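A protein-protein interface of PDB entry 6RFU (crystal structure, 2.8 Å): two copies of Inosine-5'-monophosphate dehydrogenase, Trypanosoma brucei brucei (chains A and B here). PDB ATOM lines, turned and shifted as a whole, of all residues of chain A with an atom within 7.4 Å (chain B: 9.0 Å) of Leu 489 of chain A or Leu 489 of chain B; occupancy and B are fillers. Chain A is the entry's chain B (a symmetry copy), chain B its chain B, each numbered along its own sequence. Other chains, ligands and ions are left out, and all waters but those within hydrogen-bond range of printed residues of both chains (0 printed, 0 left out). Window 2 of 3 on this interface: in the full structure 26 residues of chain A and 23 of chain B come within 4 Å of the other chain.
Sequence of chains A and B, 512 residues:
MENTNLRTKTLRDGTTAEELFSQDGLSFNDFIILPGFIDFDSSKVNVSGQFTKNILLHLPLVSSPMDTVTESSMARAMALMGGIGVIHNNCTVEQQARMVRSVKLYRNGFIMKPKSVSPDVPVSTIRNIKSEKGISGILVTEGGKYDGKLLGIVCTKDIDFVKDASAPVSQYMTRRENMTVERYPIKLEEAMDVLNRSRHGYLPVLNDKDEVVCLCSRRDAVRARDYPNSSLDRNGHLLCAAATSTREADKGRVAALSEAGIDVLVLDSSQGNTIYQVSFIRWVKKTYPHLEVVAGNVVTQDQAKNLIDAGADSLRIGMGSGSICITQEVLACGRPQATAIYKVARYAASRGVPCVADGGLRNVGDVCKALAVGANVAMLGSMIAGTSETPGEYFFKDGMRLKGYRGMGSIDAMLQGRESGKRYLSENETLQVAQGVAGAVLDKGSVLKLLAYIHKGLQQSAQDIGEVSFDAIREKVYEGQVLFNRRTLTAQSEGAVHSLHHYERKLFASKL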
ATOM      1  N   ASP A  24      30.648  11.206   6.772  1.00  0.00           N
ATOM      2  CA  ASP A  24      30.487  10.953   8.210  1.00  0.00           C
ATOM      3  C   ASP A  24      31.781  10.474   8.855  1.00  0.00           C
ATOM      4  O   ASP A  24      32.651   9.894   8.197  1.00  0.00           O
ATOM      5  CB  ASP A  24      29.410   9.891   8.486  1.00  0.00           C
ATOM      6  CG  ASP A  24      28.127  10.136   7.738  1.00  0.00           C
ATOM      7  OD1 ASP A  24      28.183  10.277   6.494  1.00  0.00           O
ATOM      8  OD2 ASP A  24      27.063  10.170   8.397  1.00  0.00           O
ATOM      9  N   GLY A  25      31.900  10.711  10.153  1.00  0.00           N
ATOM     10  CA  GLY A  25      32.918  10.050  10.939  1.00  0.00           C
ATOM     11  C   GLY A  25      32.510   8.599  11.110  1.00  0.00           C
ATOM     12  O   GLY A  25      31.423   8.322  11.618  1.00  0.00           O
ATOM     13  N   SER A  27      32.934   4.417  12.216  1.00  0.00           N
ATOM     14  CA  SER A  27      33.458   3.346  13.045  1.00  0.00           C
ATOM     15  C   SER A  27      34.011   2.265  12.135  1.00  0.00           C
ATOM     16  O   SER A  27      33.766   2.286  10.932  1.00  0.00           O
ATOM     17  CB  SER A  27      32.358   2.774  13.938  1.00  0.00           C
ATOM     18  OG  SER A  27      32.587   1.403  14.217  1.00  0.00           O
ATOM     19  N   ASP A  30      31.280   0.385  10.371  1.00  0.00           N
ATOM     20  CA  ASP A  30      30.530   1.054   9.318  1.00  0.00           C
ATOM     21  C   ASP A  30      30.933   0.563   7.929  1.00  0.00           C
ATOM     22  O   ASP A  30      30.274   0.879   6.943  1.00  0.00           O
ATOM     23  CB  ASP A  30      30.717   2.573   9.410  1.00  0.00           C
ATOM     24  CG  ASP A  30      29.804   3.216  10.443  1.00  0.00           C
ATOM     25  OD1 ASP A  30      28.579   2.955  10.426  1.00  0.00           O
ATOM     26  OD2 ASP A  30      30.316   3.988  11.276  1.00  0.00           O
ATOM     27  N   ARG A 486      30.785   0.664   2.443  1.00  0.00           N
ATOM     28  CA  ARG A 486      30.087   1.126   3.632  1.00  0.00           C
ATOM     29  C   ARG A 486      28.834   0.290   3.807  1.00  0.00           C
ATOM     30  O   ARG A 486      28.129   0.017   2.843  1.00  0.00           O
ATOM     31  CB  ARG A 486      29.731   2.610   3.530  1.00  0.00           C
ATOM     32  CG  ARG A 486      29.003   3.135   4.753  1.00  0.00           C
ATOM     33  CD  ARG A 486      28.946   4.649   4.783  1.00  0.00           C
ATOM     34  NE  ARG A 486      28.484   5.148   6.074  1.00  0.00           N
ATOM     35  CZ  ARG A 486      28.415   6.433   6.398  1.00  0.00           C
ATOM     36  NH1 ARG A 486      28.775   7.362   5.528  1.00  0.00           N
ATOM     37  NH2 ARG A 486      27.983   6.791   7.598  1.00  0.00           N
ATOM     38  N   ARG A 487      28.564  -0.128   5.035  1.00  0.00           N
ATOM     39  CA  ARG A 487      27.381  -0.924   5.314  1.00  0.00           C
ATOM     40  C   ARG A 487      26.294  -0.058   5.915  1.00  0.00           C
ATOM     41  O   ARG A 487      26.563   0.785   6.771  1.00  0.00           O
ATOM     42  CB  ARG A 487      27.708  -2.072   6.268  1.00  0.00           C
ATOM     43  CG  ARG A 487      28.676  -3.098   5.720  1.00  0.00           C
ATOM     44  CD  ARG A 487      28.728  -4.322   6.629  1.00  0.00           C
ATOM     45  NE  ARG A 487      29.269  -3.994   7.948  1.00  0.00           N
ATOM     46  CZ  ARG A 487      29.429  -4.874   8.932  1.00  0.00           C
ATOM     47  NH1 ARG A 487      29.079  -6.143   8.752  1.00  0.00           N
ATOM     48  NH2 ARG A 487      29.937  -4.484  10.098  1.00  0.00           N
ATOM     49  N   THR A 488      25.064  -0.266   5.460  1.00  0.00           N
ATOM     50  CA  THR A 488      23.914   0.334   6.116  1.00  0.00           C
ATOM     51  C   THR A 488      23.794  -0.251   7.504  1.00  0.00           C
ATOM     52  O   THR A 488      24.396  -1.274   7.811  1.00  0.00           O
ATOM     53  CB  THR A 488      22.595   0.084   5.359  1.00  0.00           C
ATOM     54  OG1 THR A 488      22.254  -1.310   5.410  1.00  0.00           O
ATOM     55  CG2 THR A 488      22.722   0.530   3.915  1.00  0.00           C
ATOM     56  N   LEU A 489      22.994   0.389   8.340  1.00  0.00           N
ATOM     57  CA  LEU A 489      22.850  -0.053   9.709  1.00  0.00           C
ATOM     58  C   LEU A 489      22.140  -1.390   9.799  1.00  0.00           C
ATOM     59  O   LEU A 489      22.448  -2.191  10.683  1.00  0.00           O
ATOM     60  CB  LEU A 489      22.114   1.006  10.515  1.00  0.00           C
ATOM     61  CG  LEU A 489      23.035   2.203  10.702  1.00  0.00           C
ATOM     62  CD1 LEU A 489      22.280   3.494  10.869  1.00  0.00           C
ATOM     63  CD2 LEU A 489      23.923   1.952  11.893  1.00  0.00           C
ATOM     64  N   THR A 490      21.207  -1.650   8.888  1.00  0.00           N
ATOM     65  CA  THR A 490      20.486  -2.916   8.930  1.00  0.00           C
ATOM     66  C   THR A 490      21.347  -4.006   8.297  1.00  0.00           C
ATOM     67  O   THR A 490      21.176  -5.191   8.583  1.00  0.00           O
ATOM     68  CB  THR A 490      19.127  -2.855   8.215  1.00  0.00           C
ATOM     69  OG1 THR A 490      19.293  -3.177   6.830  1.00  0.00           O
ATOM     70  CG2 THR A 490      18.508  -1.488   8.366  1.00  0.00           C
ATOM     71  N   ALA A 491      22.279  -3.602   7.440  1.00  0.00           N
ATOM     72  CA  ALA A 491      23.226  -4.544   6.860  1.00  0.00           C
ATOM     73  C   ALA A 491      24.234  -4.971   7.924  1.00  0.00           C
ATOM     74  O   ALA A 491      24.888  -6.007   7.798  1.00  0.00           O
ATOM     75  CB  ALA A 491      23.933  -3.930   5.663  1.00  0.00           C
ATOM     76  N   GLN A 492      24.354  -4.163   8.973  1.00  0.00           N
ATOM     77  CA  GLN A 492      25.247  -4.471  10.082  1.00  0.00           C
ATOM     78  C   GLN A 492      24.596  -5.386  11.119  1.00  0.00           C
ATOM     79  O   GLN A 492      25.275  -5.910  12.006  1.00  0.00           O
ATOM     80  CB  GLN A 492      25.706  -3.182  10.754  1.00  0.00           C
ATOM     81  CG  GLN A 492      26.626  -2.343   9.904  1.00  0.00           C
ATOM     82  CD  GLN A 492      27.000  -1.049  10.586  1.00  0.00           C
ATOM     83  OE1 GLN A 492      27.345  -1.042  11.770  1.00  0.00           O
ATOM     84  NE2 GLN A 492      26.931   0.056   9.851  1.00  0.00           N
ATOM     85  N   SER A 493      23.282  -5.569  11.003  1.00  0.00           N
ATOM     86  CA  SER A 493      22.521  -6.400  11.936  1.00  0.00           C
ATOM     87  C   SER A 493      22.209  -7.762  11.330  1.00  0.00           C
ATOM     88  O   SER A 493      21.049  -8.173  11.279  1.00  0.00           O
ATOM     89  CB  SER A 493      21.224  -5.699  12.330  1.00  0.00           C
ATOM     90  OG  SER A 493      21.480  -4.365  12.733  1.00  0.00           O
ATOM     91  N   GLU A 494      23.254  -8.451  10.875  1.00  0.00           N
ATOM     92  CA  GLU A 494      23.120  -9.760  10.236  1.00  0.00           C
ATOM     93  C   GLU A 494      24.444 -10.210   9.612  1.00  0.00           C
ATOM     94  O   GLU A 494      25.505  -9.640   9.887  1.00  0.00           O
ATOM     95  CB  GLU A 494      22.016  -9.729   9.171  1.00  0.00           C
ATOM     96  CG  GLU A 494      22.091  -8.542   8.209  1.00  0.00           C
ATOM     97  CD  GLU A 494      20.743  -8.216   7.570  1.00  0.00           C
ATOM     98  OE1 GLU A 494      20.709  -7.913   6.356  1.00  0.00           O
ATOM     99  OE2 GLU A 494      19.715  -8.256   8.284  1.00  0.00           O
ATOM    100  N   ASP B  24      20.432  17.138   7.456  1.00  0.00           N
ATOM    101  CA  ASP B  24      19.503  16.665   8.493  1.00  0.00           C
ATOM    102  C   ASP B  24      19.420  17.630   9.669  1.00  0.00           C
ATOM    103  O   ASP B  24      20.355  18.388   9.946  1.00  0.00           O
ATOM    104  CB  ASP B  24      19.917  15.292   9.047  1.00  0.00           C
ATOM    105  CG  ASP B  24      20.231  14.286   7.971  1.00  0.00           C
ATOM    106  OD1 ASP B  24      21.079  14.593   7.101  1.00  0.00           O
ATOM    107  OD2 ASP B  24      19.639  13.183   8.010  1.00  0.00           O
ATOM    108  N   SER B  27      20.932  16.345  16.405  1.00  0.00           N
ATOM    109  CA  SER B  27      21.045  16.379  17.853  1.00  0.00           C
ATOM    110  C   SER B  27      22.476  16.735  18.212  1.00  0.00           C
ATOM    111  O   SER B  27      23.352  16.717  17.351  1.00  0.00           O
ATOM    112  CB  SER B  27      20.671  15.023  18.450  1.00  0.00           C
ATOM    113  OG  SER B  27      21.375  14.785  19.658  1.00  0.00           O
ATOM    114  N   ASN B  29      24.263  14.896  19.919  1.00  0.00           N
ATOM    115  CA  ASN B  29      24.955  13.618  19.882  1.00  0.00           C
ATOM    116  C   ASN B  29      25.430  13.271  18.489  1.00  0.00           C
ATOM    117  O   ASN B  29      26.321  12.440  18.327  1.00  0.00           O
ATOM    118  CB  ASN B  29      24.055  12.508  20.412  1.00  0.00           C
ATOM    119  CG  ASN B  29      24.103  12.403  21.918  1.00  0.00           C
ATOM    120  OD1 ASN B  29      23.311  13.032  22.624  1.00  0.00           O
ATOM    121  ND2 ASN B  29      25.053  11.621  22.424  1.00  0.00           N
ATOM    122  N   ASP B  30      24.847  13.914  17.485  1.00  0.00           N
ATOM    123  CA  ASP B  30      25.150  13.588  16.099  1.00  0.00           C
ATOM    124  C   ASP B  30      26.545  14.059  15.694  1.00  0.00           C
ATOM    125  O   ASP B  30      27.035  13.702  14.626  1.00  0.00           O
ATOM    126  CB  ASP B  30      24.100  14.198  15.163  1.00  0.00           C
ATOM    127  CG  ASP B  30      22.838  13.352  15.067  1.00  0.00           C
ATOM    128  OD1 ASP B  30      22.938  12.127  14.828  1.00  0.00           O
ATOM    129  OD2 ASP B  30      21.741  13.919  15.230  1.00  0.00           O
ATOM    130  N   ARG B 486      30.600  14.889  12.088  1.00  0.00           N
ATOM    131  CA  ARG B 486      29.354  14.166  12.288  1.00  0.00           C
ATOM    132  C   ARG B 486      29.683  12.712  12.562  1.00  0.00           C
ATOM    133  O   ARG B 486      30.539  12.133  11.903  1.00  0.00           O
ATOM    134  CB  ARG B 486      28.435  14.288  11.071  1.00  0.00           C
ATOM    135  CG  ARG B 486      27.121  13.550  11.239  1.00  0.00           C
ATOM    136  CD  ARG B 486      26.103  13.939  10.186  1.00  0.00           C
ATOM    137  NE  ARG B 486      24.773  13.431  10.505  1.00  0.00           N
ATOM    138  CZ  ARG B 486      23.683  13.691   9.793  1.00  0.00           C
ATOM    139  NH1 ARG B 486      23.756  14.453   8.714  1.00  0.00           N
ATOM    140  NH2 ARG B 486      22.516  13.186  10.162  1.00  0.00           N
ATOM    141  N   ARG B 487      29.013  12.124  13.542  1.00  0.00           N
ATOM    142  CA  ARG B 487      29.243  10.729  13.878  1.00  0.00           C
ATOM    143  C   ARG B 487      28.149   9.860  13.293  1.00  0.00           C
ATOM    144  O   ARG B 487      26.971  10.216  13.340  1.00  0.00           O
ATOM    145  CB  ARG B 487      29.299  10.533  15.392  1.00  0.00           C
ATOM    146  CG  ARG B 487      30.449  11.234  16.082  1.00  0.00           C
ATOM    147  CD  ARG B 487      30.569  10.764  17.529  1.00  0.00           C
ATOM    148  NE  ARG B 487      29.398  11.144  18.320  1.00  0.00           N
ATOM    149  CZ  ARG B 487      29.244  10.865  19.611  1.00  0.00           C
ATOM    150  NH1 ARG B 487      30.187  10.193  20.262  1.00  0.00           N
ATOM    151  NH2 ARG B 487      28.146  11.259  20.250  1.00  0.00           N
ATOM    152  N   THR B 488      28.543   8.721  12.737  1.00  0.00           N
ATOM    153  CA  THR B 488      27.577   7.706  12.351  1.00  0.00           C
ATOM    154  C   THR B 488      26.907   7.182  13.600  1.00  0.00           C
ATOM    155  O   THR B 488      27.386   7.392  14.709  1.00  0.00           O
ATOM    156  CB  THR B 488      28.220   6.521  11.603  1.00  0.00           C
ATOM    157  OG1 THR B 488      29.071   5.780  12.491  1.00  0.00           O
ATOM    158  CG2 THR B 488      29.024   7.020  10.418  1.00  0.00           C
ATOM    159  N   LEU B 489      25.803   6.477  13.418  1.00  0.00           N
ATOM    160  CA  LEU B 489      25.051   5.976  14.547  1.00  0.00           C
ATOM    161  C   LEU B 489      25.810   4.897  15.297  1.00  0.00           C
ATOM    162  O   LEU B 489      25.690   4.799  16.519  1.00  0.00           O
ATOM    163  CB  LEU B 489      23.701   5.460  14.077  1.00  0.00           C
ATOM    164  CG  LEU B 489      22.840   6.647  13.670  1.00  0.00           C
ATOM    165  CD1 LEU B 489      21.818   6.291  12.625  1.00  0.00           C
ATOM    166  CD2 LEU B 489      22.169   7.203  14.899  1.00  0.00           C
ATOM    167  N   THR B 490      26.602   4.100  14.587  1.00  0.00           N
ATOM    168  CA  THR B 490      27.350   3.041  15.253  1.00  0.00           C
ATOM    169  C   THR B 490      28.599   3.636  15.897  1.00  0.00           C
ATOM    170  O   THR B 490      29.147   3.076  16.847  1.00  0.00           O
ATOM    171  CB  THR B 490      27.754   1.904  14.301  1.00  0.00           C
ATOM    172  OG1 THR B 490      29.019   2.202  13.701  1.00  0.00           O
ATOM    173  CG2 THR B 490      26.704   1.701  13.239  1.00  0.00           C
ATOM    174  N   ALA B 491      29.044   4.778  15.383  1.00  0.00           N
ATOM    175  CA  ALA B 491      30.162   5.489  15.988  1.00  0.00           C
ATOM    176  C   ALA B 491      29.710   6.127  17.299  1.00  0.00           C
ATOM    177  O   ALA B 491      30.527   6.458  18.158  1.00  0.00           O
ATOM    178  CB  ALA B 491      30.710   6.540  15.037  1.00  0.00           C
ATOM    179  N   GLN B 492      28.400   6.299  17.443  1.00  0.00           N
ATOM    180  CA  GLN B 492      27.827   6.858  18.661  1.00  0.00           C
ATOM    181  C   GLN B 492      27.600   5.798  19.738  1.00  0.00           C
ATOM    182  O   GLN B 492      27.322   6.129  20.894  1.00  0.00           O
ATOM    183  CB  GLN B 492      26.509   7.555  18.344  1.00  0.00           C
ATOM    184  CG  GLN B 492      26.664   8.814  17.528  1.00  0.00           C
ATOM    185  CD  GLN B 492      25.329   9.432  17.187  1.00  0.00           C
ATOM    186  OE1 GLN B 492      24.456   9.555  18.049  1.00  0.00           O
ATOM    187  NE2 GLN B 492      25.155   9.819  15.928  1.00  0.00           N
ATOM    188  N   SER B 493      27.717   4.529  19.352  1.00  0.00           N
ATOM    189  CA  SER B 493      27.506   3.408  20.269  1.00  0.00           C
ATOM    190  C   SER B 493      28.832   2.816  20.727  1.00  0.00           C
ATOM    191  O   SER B 493      29.060   1.613  20.592  1.00  0.00           O
ATOM    192  CB  SER B 493      26.661   2.329  19.598  1.00  0.00           C
ATOM    193  OG  SER B 493      25.502   2.896  19.011  1.00  0.00           O
ATOM    194  N   GLU B 494      29.697   3.672  21.267  1.00  0.00           N
ATOM    195  CA  GLU B 494      31.026   3.269  21.727  1.00  0.00           C
ATOM    196  C   GLU B 494      31.881   4.486  22.088  1.00  0.00           C
ATOM    197  O   GLU B 494      31.374   5.605  22.220  1.00  0.00           O
ATOM    198  CB  GLU B 494      31.732   2.422  20.659  1.00  0.00           C
ATOM    199  CG  GLU B 494      31.685   3.009  19.247  1.00  0.00           C
ATOM    200  CD  GLU B 494      31.860   1.947  18.163  1.00  0.00           C
ATOM    201  OE1 GLU B 494      32.573   2.213  17.170  1.00  0.00           O
ATOM    202  OE2 GLU B 494      31.278   0.847  18.301  1.00  0.00           O
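Hydrophobic or aromatic side chains of chain B within 4 Å of the printed part of chain A: Leu 489 and Ala 491. Of the 13 printed residues of chain A, 7 touch a printed residue of chain B. Among the printed residues, 14 pairs touch across the chains.
Asp 24 of chain A touches Arg 486 of chain B, but with the chains exchanged Arg 486 of chain A does not touch Asp 24 of chain B (10.4 Å). Asp 24 of chain A touches Thr 488 of chain B, but with the chains exchanged Thr 488 of chain A does not touch Asp 24 of chain B (13.7 Å). Arg 486 of chain A touches Thr 488 of chain B, but with the chains exchanged Thr 488 of chain A does not touch Arg 486 of chain B (13.5 Å). Leu 489 of chain A touches its own counterpart, Leu 489 of chain B. Positions printed for both chains: 24, 27, 30, 486, 487, 488, 489, 490, 491, 492, 493 and 494. Of the 14 pairs that touch across the chains among the printed residues, 1 has its exchanged pair printed and touching as well.
OE1 of Glu 494 of chain B sits at hydrogen-bond distance from OG of Ser 27 of chain A. OD2 of Asp 30 of chain A is in hydrogen-bond range of OG1 of Thr 490 of chain B. O of Arg 486 of chain B sits at hydrogen-bond distance from N of Gly 25 of chain A (2.6 Å). O of Gly 25 of chain A lies close to N of Thr 488 of chain B (3.1 Å). The side-chain hydroxyl (OG1) of Thr 488 of chain B sits at hydrogen-bond distance from the side-chain carboxylate (OD2) of Asp 30 of chain A (2.5 Å).
Arg 486 of chain B touches Asp 24 of chain A (O to C, 3.7 Å). Thr 488 of chain B touches Asp 24 of chain A. Arg 487 of chain B touches Gly 25 of chain A (CA to O, 3.96 Å). Gly 25 of chain A touches Ala 491 of chain B (O to CB, 3.9 Å). Ser 27 of chain A touches Thr 490 of chain B (CB to OG1, 3.4 Å). Arg 486 of chain A touches Thr 488 of chain B (NH2 to CG2, 3.0 Å). Leu 489 of chain B touches Leu 489 of chain A (CD1 to CD1, 3.3 Å). Leu 489 of chain A touches Thr 490 of chain B (CD2 to CG2, 3.1 Å). Gln 492 of chain A touches Thr 490 of chain B.
Printed residues of chain B within 4 Å of Asp 30 of chain A: Thr 488 and Thr 490. Of the printed residues of chain B, Arg 486 of chain A touches Thr 488 (3.0 Å). Thr 488 of chain A touches none of the printed residues of chain B. No residue of chain B comes within 4 Å of Thr 490 of chain A. Printed residues of chain B within 4 Å of Gln 492 of chain A: Thr 490 (3.2 Å). Asp 24 of chain B touches none of the printed residues of chain A. Of the printed residues of chain A, Arg 487 of chain B touches Gly 25. Printed residues of chain A within 4 Å of Leu 489 of chain B: Leu 489 (3.3 Å). The nearest residue of chain A that does not touch Leu 489 of chain B is Asp 30 of chain A (5.4 Å).
The backbone carbonyl oxygen (O) of Asn 29 of chain B is in hydrogen-bond range of the guanidinium group (NH2) of Arg 487 of chain B (2.9 Å). The side-chain amide nitrogen (NE2) of Gln 492 of chain A lies within hydrogen-bond range of the side-chain carboxylate (OD1) of Asp 30 of chain A (3.4 Å). The backbone carbonyl oxygen of Arg 487 of chain A is in hydrogen-bond range of the side-chain amide nitrogen of Gln 492 of chain A (3.2 Å). The side-chain carboxylate of Asp 24 of chain A lies within salt-bridge range of the guanidinium group of Arg 486 of chain A (3.1 Å). The side-chain hydroxyl (OG) of Ser 493 of chain A is in hydrogen-bond range of the backbone carbonyl oxygen (O) of Leu 489 of chain A (3.1 Å). The backbone carbonyl oxygen (O) of Arg 487 of chain B sits at hydrogen-bond distance from the side-chain amide nitrogen (NE2) of Gln 492 of chain B (3.2 Å).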
